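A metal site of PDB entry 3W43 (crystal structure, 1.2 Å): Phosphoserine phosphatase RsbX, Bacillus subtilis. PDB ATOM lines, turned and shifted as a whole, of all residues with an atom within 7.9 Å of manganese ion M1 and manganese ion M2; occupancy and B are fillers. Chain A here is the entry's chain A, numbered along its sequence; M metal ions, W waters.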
ATOM      1  N   LYS A  19       9.068 -19.620  32.637  1.00  0.00           N
ATOM      2  CA  LYS A  19       8.337 -18.454  33.054  1.00  0.00           C
ATOM      3  C   LYS A  19       6.845 -18.794  33.178  1.00  0.00           C
ATOM      4  O   LYS A  19       6.309 -19.623  32.436  1.00  0.00           O
ATOM      5  CB  LYS A  19       8.511 -17.359  32.019  1.00  0.00           C
ATOM      6  CG  LYS A  19       7.878 -16.063  32.421  1.00  0.00           C
ATOM      7  CD  LYS A  19       8.143 -14.984  31.424  1.00  0.00           C
ATOM      8  CE  LYS A  19       7.566 -13.683  31.934  1.00  0.00           C
ATOM      9  NZ  LYS A  19       8.029 -12.562  31.094  1.00  0.00           N
ATOM     10  N   CYS A  25      10.274 -23.254  27.038  1.00  0.00           N
ATOM     11  CA  CYS A  25      11.262 -22.438  27.709  1.00  0.00           C
ATOM     12  C   CYS A  25      12.084 -21.622  26.738  1.00  0.00           C
ATOM     13  O   CYS A  25      12.560 -22.122  25.716  1.00  0.00           O
ATOM     14  CB  CYS A  25      12.178 -23.337  28.534  1.00  0.00           C
ATOM     15  SG  CYS A  25      13.135 -22.448  29.783  1.00  0.00           S
ATOM     16  N   GLY A  26      12.249 -20.338  27.046  1.00  0.00           N
ATOM     17  CA  GLY A  26      13.143 -19.495  26.266  1.00  0.00           C
ATOM     18  C   GLY A  26      14.613 -19.773  26.511  1.00  0.00           C
ATOM     19  O   GLY A  26      15.444 -19.393  25.694  1.00  0.00           O
ATOM     20  N   ASP A  27      14.934 -20.435  27.625  1.00  0.00           N
ATOM     21  CA  ASP A  27      16.303 -20.870  27.905  1.00  0.00           C
ATOM     22  C   ASP A  27      16.517 -22.246  27.282  1.00  0.00           C
ATOM     23  O   ASP A  27      15.564 -23.048  27.240  1.00  0.00           O
ATOM     24  CB  ASP A  27      16.534 -21.079  29.412  1.00  0.00           C
ATOM     25  CG  ASP A  27      16.470 -19.804  30.259  1.00  0.00           C
ATOM     26  OD1 ASP A  27      16.400 -18.654  29.746  1.00  0.00           O
ATOM     27  OD2 ASP A  27      16.493 -20.010  31.498  1.00  0.00           O
ATOM     28  N   ALA A  43      21.940 -21.170  27.441  1.00  0.00           N
ATOM     29  CA  ALA A  43      21.579 -19.998  26.647  1.00  0.00           C
ATOM     30  C   ALA A  43      20.204 -19.482  27.026  1.00  0.00           C
ATOM     31  O   ALA A  43      19.288 -20.245  27.304  1.00  0.00           O
ATOM     32  CB  ALA A  43      21.615 -20.344  25.169  1.00  0.00           C
ATOM     33  N   ASP A  44      20.071 -18.157  27.030  1.00  0.00           N
ATOM     34  CA  ASP A  44      18.819 -17.493  27.354  1.00  0.00           C
ATOM     35  C   ASP A  44      18.411 -16.662  26.132  1.00  0.00           C
ATOM     36  O   ASP A  44      19.019 -15.656  25.831  1.00  0.00           O
ATOM     37  CB  ASP A  44      19.062 -16.604  28.581  1.00  0.00           C
ATOM     38  CG  ASP A  44      17.818 -15.831  29.003  1.00  0.00           C
ATOM     39  OD1 ASP A  44      16.804 -15.906  28.272  1.00  0.00           O
ATOM     40  OD2 ASP A  44      17.842 -15.168  30.063  1.00  0.00           O
ATOM     41  N   GLY A  45      17.405 -17.150  25.395  1.00  0.00           N
ATOM     42  CA  GLY A  45      16.935 -16.431  24.212  1.00  0.00           C
ATOM     43  C   GLY A  45      16.244 -15.156  24.649  1.00  0.00           C
ATOM     44  O   GLY A  45      15.582 -15.133  25.669  1.00  0.00           O
ATOM     45  N   LEU A  46      16.425 -14.096  23.884  1.00  0.00           N
ATOM     46  CA  LEU A  46      15.778 -12.826  24.241  1.00  0.00           C
ATOM     47  C   LEU A  46      14.272 -12.986  24.358  1.00  0.00           C
ATOM     48  O   LEU A  46      13.636 -13.637  23.533  1.00  0.00           O
ATOM     49  CB  LEU A  46      16.147 -11.741  23.248  1.00  0.00           C
ATOM     50  CG  LEU A  46      17.365 -10.901  23.632  1.00  0.00           C
ATOM     51  CD1 LEU A  46      18.645 -11.691  23.850  1.00  0.00           C
ATOM     52  CD2 LEU A  46      17.561  -9.812  22.598  1.00  0.00           C
ATOM     53  N   GLY A  47      13.711 -12.395  25.413  1.00  0.00           N
ATOM     54  CA  GLY A  47      12.304 -12.565  25.724  1.00  0.00           C
ATOM     55  C   GLY A  47      12.052 -13.916  26.347  1.00  0.00           C
ATOM     56  O   GLY A  47      12.891 -14.452  27.101  1.00  0.00           O
ATOM     57  N   SER A  48      10.908 -14.501  26.025  1.00  0.00           N
ATOM     58  CA  SER A  48      10.529 -15.801  26.580  1.00  0.00           C
ATOM     59  C   SER A  48       9.745 -16.571  25.531  1.00  0.00           C
ATOM     60  O   SER A  48       9.526 -16.089  24.433  1.00  0.00           O
ATOM     61  CB  SER A  48       9.725 -15.649  27.871  1.00  0.00           C
ATOM     62  OG  SER A  48       8.488 -14.987  27.645  1.00  0.00           O
ATOM     63  N   GLY A  49       9.336 -17.788  25.871  1.00  0.00           N
ATOM     64  CA  GLY A  49       8.444 -18.550  24.999  1.00  0.00           C
ATOM     65  C   GLY A  49       9.076 -18.974  23.694  1.00  0.00           C
ATOM     66  O   GLY A  49      10.297 -19.128  23.590  1.00  0.00           O
ATOM     67  N   ALA A  52      11.952 -16.838  21.936  1.00  0.00           N
ATOM     68  CA  ALA A  52      13.217 -16.960  22.680  1.00  0.00           C
ATOM     69  C   ALA A  52      13.841 -18.321  22.423  1.00  0.00           C
ATOM     70  O   ALA A  52      15.060 -18.435  22.188  1.00  0.00           O
ATOM     71  CB  ALA A  52      12.943 -16.775  24.147  1.00  0.00           C
ATOM     72  N   ASN A  53      13.002 -19.361  22.443  1.00  0.00           N
ATOM     73  CA  ASN A  53      13.446 -20.721  22.222  1.00  0.00           C
ATOM     74  C   ASN A  53      14.060 -20.896  20.830  1.00  0.00           C
ATOM     75  O   ASN A  53      15.037 -21.615  20.676  1.00  0.00           O
ATOM     76  CB  ASN A  53      12.301 -21.707  22.456  1.00  0.00           C
ATOM     77  CG  ASN A  53      12.743 -23.138  22.302  1.00  0.00           C
ATOM     78  OD1 ASN A  53      12.667 -23.697  21.219  1.00  0.00           O
ATOM     79  ND2 ASN A  53      13.245 -23.727  23.379  1.00  0.00           N
ATOM     80  N   SER A  56      17.671 -19.788  21.486  1.00  0.00           N
ATOM     81  CA  SER A  56      18.473 -20.612  22.393  1.00  0.00           C
ATOM     82  C   SER A  56      18.596 -22.061  21.933  1.00  0.00           C
ATOM     83  O   SER A  56      19.632 -22.686  22.139  1.00  0.00           O
ATOM     84  CB  SER A  56      17.953 -20.518  23.822  1.00  0.00           C
ATOM     85  OG  SER A  56      16.650 -21.068  23.921  1.00  0.00           O
ATOM     86  N   ARG A  86      15.893 -13.504  17.243  1.00  0.00           N
ATOM     87  CA  ARG A  86      15.908 -12.520  18.326  1.00  0.00           C
ATOM     88  C   ARG A  86      17.315 -12.356  18.890  1.00  0.00           C
ATOM     89  O   ARG A  86      17.740 -11.249  19.221  1.00  0.00           O
ATOM     90  CB  ARG A  86      14.959 -12.906  19.458  1.00  0.00           C
ATOM     91  CG  ARG A  86      13.497 -12.574  19.234  1.00  0.00           C
ATOM     92  CD  ARG A  86      12.700 -12.882  20.488  1.00  0.00           C
ATOM     93  NE  ARG A  86      11.334 -12.389  20.471  1.00  0.00           N
ATOM     94  CZ  ARG A  86      10.467 -12.581  21.466  1.00  0.00           C
ATOM     95  NH1 ARG A  86      10.833 -13.274  22.532  1.00  0.00           N
ATOM     96  NH2 ARG A  86       9.235 -12.113  21.385  1.00  0.00           N
ATOM     97  N   GLY A  87      18.028 -13.479  19.020  1.00  0.00           N
ATOM     98  CA  GLY A  87      19.320 -13.465  19.689  1.00  0.00           C
ATOM     99  C   GLY A  87      19.249 -14.060  21.073  1.00  0.00           C
ATOM    100  O   GLY A  87      18.160 -14.406  21.552  1.00  0.00           O
ATOM    101  N   ALA A  88      20.400 -14.191  21.729  1.00  0.00           N
ATOM    102  CA  ALA A  88      20.452 -14.868  23.014  1.00  0.00           C
ATOM    103  C   ALA A  88      21.686 -14.455  23.773  1.00  0.00           C
ATOM    104  O   ALA A  88      22.671 -14.032  23.171  1.00  0.00           O
ATOM    105  CB  ALA A  88      20.467 -16.387  22.813  1.00  0.00           C
ATOM    106  N   THR A  89      21.646 -14.619  25.095  1.00  0.00           N
ATOM    107  CA  THR A  89      22.846 -14.596  25.913  1.00  0.00           C
ATOM    108  C   THR A  89      23.272 -16.055  26.156  1.00  0.00           C
ATOM    109  O   THR A  89      22.437 -16.963  26.102  1.00  0.00           O
ATOM    110  CB  THR A  89      22.597 -13.838  27.224  1.00  0.00           C
ATOM    111  OG1 THR A  89      21.506 -14.468  27.919  1.00  0.00           O
ATOM    112  CG2 THR A  89      22.223 -12.382  26.927  1.00  0.00           C
ATOM    113  N   ASN A 109      24.029 -11.944  30.419  1.00  0.00           N
ATOM    114  CA  ASN A 109      23.836 -12.262  31.829  1.00  0.00           C
ATOM    115  C   ASN A 109      23.497 -13.730  32.097  1.00  0.00           C
ATOM    116  O   ASN A 109      22.452 -14.070  32.666  1.00  0.00           O
ATOM    117  CB  ASN A 109      22.757 -11.346  32.452  1.00  0.00           C
ATOM    118  CG  ASN A 109      22.777 -11.362  33.978  1.00  0.00           C
ATOM    119  OD1 ASN A 109      23.740 -11.826  34.609  1.00  0.00           O
ATOM    120  ND2 ASN A 109      21.712 -10.839  34.592  1.00  0.00           N
ATOM    121  N   VAL A 110      24.395 -14.617  31.665  1.00  0.00           N
ATOM    122  CA  VAL A 110      24.408 -15.998  32.093  1.00  0.00           C
ATOM    123  C   VAL A 110      25.683 -16.096  32.929  1.00  0.00           C
ATOM    124  O   VAL A 110      26.760 -15.702  32.464  1.00  0.00           O
ATOM    125  CB  VAL A 110      24.428 -16.972  30.887  1.00  0.00           C
ATOM    126  CG1 VAL A 110      24.404 -18.419  31.364  1.00  0.00           C
ATOM    127  CG2 VAL A 110      23.236 -16.727  29.942  1.00  0.00           C
ATOM    128  N   THR A 155      21.014 -19.071  34.258  1.00  0.00           N
ATOM    129  CA  THR A 155      20.407 -17.909  33.634  1.00  0.00           C
ATOM    130  C   THR A 155      19.912 -16.910  34.663  1.00  0.00           C
ATOM    131  O   THR A 155      19.861 -17.176  35.872  1.00  0.00           O
ATOM    132  CB  THR A 155      19.272 -18.293  32.660  1.00  0.00           C
ATOM    133  OG1 THR A 155      18.216 -18.946  33.391  1.00  0.00           O
ATOM    134  CG2 THR A 155      19.790 -19.197  31.553  1.00  0.00           C
ATOM    135  N   ASP A 156      19.563 -15.728  34.163  1.00  0.00           N
ATOM    136  CA  ASP A 156      19.165 -14.610  35.006  1.00  0.00           C
ATOM    137  C   ASP A 156      17.800 -14.787  35.677  1.00  0.00           C
ATOM    138  O   ASP A 156      17.414 -13.980  36.497  1.00  0.00           O
ATOM    139  CB  ASP A 156      19.272 -13.295  34.217  1.00  0.00           C
ATOM    140  CG  ASP A 156      18.376 -13.262  32.988  1.00  0.00           C
ATOM    141  OD1 ASP A 156      17.456 -14.096  32.880  1.00  0.00           O
ATOM    142  OD2 ASP A 156      18.599 -12.368  32.122  1.00  0.00           O
ATOM    143  N   GLY A 157      17.073 -15.848  35.342  1.00  0.00           N
ATOM    144  CA  GLY A 157      15.882 -16.202  36.087  1.00  0.00           C
ATOM    145  C   GLY A 157      16.211 -16.610  37.508  1.00  0.00           C
ATOM    146  O   GLY A 157      15.350 -16.577  38.367  1.00  0.00           O
ATOM    147  N   LEU A 158      17.452 -17.029  37.753  1.00  0.00           N
ATOM    148  CA  LEU A 158      17.931 -17.365  39.089  1.00  0.00           C
ATOM    149  C   LEU A 158      18.717 -16.177  39.623  1.00  0.00           C
ATOM    150  O   LEU A 158      19.762 -15.803  39.066  1.00  0.00           O
ATOM    151  CB  LEU A 158      18.796 -18.627  39.072  1.00  0.00           C
ATOM    152  CG  LEU A 158      19.348 -19.072  40.432  1.00  0.00           C
ATOM    153  CD1 LEU A 158      18.226 -19.611  41.292  1.00  0.00           C
ATOM    154  CD2 LEU A 158      20.424 -20.120  40.279  1.00  0.00           C
ATOM    155  N   LYS A 188       8.998 -15.774  37.615  1.00  0.00           N
ATOM    156  CA  LYS A 188       9.010 -14.455  36.997  1.00  0.00           C
ATOM    157  C   LYS A 188       9.707 -14.475  35.645  1.00  0.00           C
ATOM    158  O   LYS A 188       9.393 -13.666  34.768  1.00  0.00           O
ATOM    159  CB  LYS A 188       9.624 -13.393  37.914  1.00  0.00           C
ATOM    160  CG  LYS A 188       8.771 -13.024  39.125  1.00  0.00           C
ATOM    161  CD  LYS A 188       9.398 -11.891  39.933  1.00  0.00           C
ATOM    162  CE  LYS A 188       9.202 -10.524  39.289  1.00  0.00           C
ATOM    163  NZ  LYS A 188       7.773 -10.074  39.289  1.00  0.00           N
ATOM    164  N   ASP A 189      10.644 -15.394  35.487  1.00  0.00           N
ATOM    165  CA  ASP A 189      11.339 -15.576  34.219  1.00  0.00           C
ATOM    166  C   ASP A 189      11.655 -17.047  34.073  1.00  0.00           C
ATOM    167  O   ASP A 189      11.612 -17.788  35.052  1.00  0.00           O
ATOM    168  CB  ASP A 189      12.644 -14.753  34.234  1.00  0.00           C
ATOM    169  CG  ASP A 189      13.338 -14.710  32.883  1.00  0.00           C
ATOM    170  OD1 ASP A 189      12.694 -15.041  31.849  1.00  0.00           O
ATOM    171  OD2 ASP A 189      14.531 -14.328  32.853  1.00  0.00           O
ATOM    172  N   ASP A 190      11.982 -17.472  32.860  1.00  0.00           N
ATOM    173  CA  ASP A 190      12.618 -18.765  32.644  1.00  0.00           C
ATOM    174  C   ASP A 190      13.821 -18.859  33.570  1.00  0.00           C
ATOM    175  O   ASP A 190      14.585 -17.903  33.724  1.00  0.00           O
ATOM    176  CB  ASP A 190      13.096 -18.904  31.196  1.00  0.00           C
ATOM    177  CG  ASP A 190      11.953 -18.935  30.188  1.00  0.00           C
ATOM    178  OD1 ASP A 190      10.901 -19.560  30.460  1.00  0.00           O
ATOM    179  OD2 ASP A 190      12.123 -18.352  29.102  1.00  0.00           O
ATOM    180  N   LEU A 191      14.011 -20.037  34.152  1.00  0.00           N
ATOM    181  CA  LEU A 191      15.086 -20.249  35.109  1.00  0.00           C
ATOM    182  C   LEU A 191      15.771 -21.580  34.814  1.00  0.00           C
ATOM    183  O   LEU A 191      15.111 -22.627  34.822  1.00  0.00           O
ATOM    184  CB  LEU A 191      14.503 -20.225  36.529  1.00  0.00           C
ATOM    185  CG  LEU A 191      15.440 -20.191  37.722  1.00  0.00           C
ATOM    186  CD1 LEU A 191      14.664 -19.786  38.949  1.00  0.00           C
ATOM    187  CD2 LEU A 191      16.114 -21.531  37.925  1.00  0.00           C
ATOM    188  N   THR A 192      17.072 -21.535  34.536  1.00  0.00           N
ATOM    189  CA  THR A 192      17.863 -22.720  34.214  1.00  0.00           C
ATOM    190  C   THR A 192      19.160 -22.666  34.989  1.00  0.00           C
ATOM    191  O   THR A 192      19.831 -21.629  35.001  1.00  0.00           O
ATOM    192  CB  THR A 192      18.202 -22.760  32.711  1.00  0.00           C
ATOM    193  OG1 THR A 192      17.000 -22.668  31.949  1.00  0.00           O
ATOM    194  CG2 THR A 192      18.903 -24.058  32.332  1.00  0.00           C
HETATM  195 MN    MN M   1      16.134 -14.620  31.286  1.00  0.00          MN
HETATM  196 MN    MN M   2      14.900 -15.073  27.819  1.00  0.00          MN
HETATM  197  O   HOH W   1      14.387 -17.194  28.285  1.00  0.00           O
HETATM  198  O   HOH W   2      16.042 -16.757  31.737  1.00  0.00           O
HETATM  199  O   HOH W   3      15.959 -13.037  27.991  1.00  0.00           O
HETATM  200  O   HOH W   4      14.443 -14.627  29.879  1.00  0.00           O
HETATM  201  O   HOH W   5      16.349 -12.477  30.698  1.00  0.00           O
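N of Asp 44 lies within hydrogen-bond range of O of Thr 89 (2.8 Å). N of Gly 45 lies within hydrogen-bond range of O of Gly 26 (3.0 Å).
Of the 29 residues printed, 3 come within 4 Å of manganese ion M1.
Of the 29 residues printed, 3 come within 4 Å of manganese ion M2.
OD1 of Asp 156 is bound to manganese ion M1. OD2 of Asp 44 binds manganese ion M1 (2.2 Å). Manganese ion M1 is bound by water W2 (2.2 Å). Water W4 is bound to manganese ion M1. Manganese ion M1 is bound by water W5, 2.2 Å away. Manganese ion M1 is bound by the side-chain carboxylate (OD2) of Asp 189. Manganese ion M1 has six donor atoms within binding distance.
Manganese ion M2 is bound by OD1 of Asp 44 (2.1 Å), water W4 (2.2 Å), O of Gly 47 (2.2 Å), water W1 (2.2 Å), O of Gly 45 (2.3 Å) and water W3 (2.3 Å). Manganese ion M2 has six donor atoms within binding distance.
Water W2 lies within hydrogen-bond range of O of Asp 190 (2.7 Å) and OD1 of Asp 27 (2.8 Å). Water W1 bridges OD2 of Asp 190 (2.7 Å) and OD1 of Asp 27 (2.9 Å).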
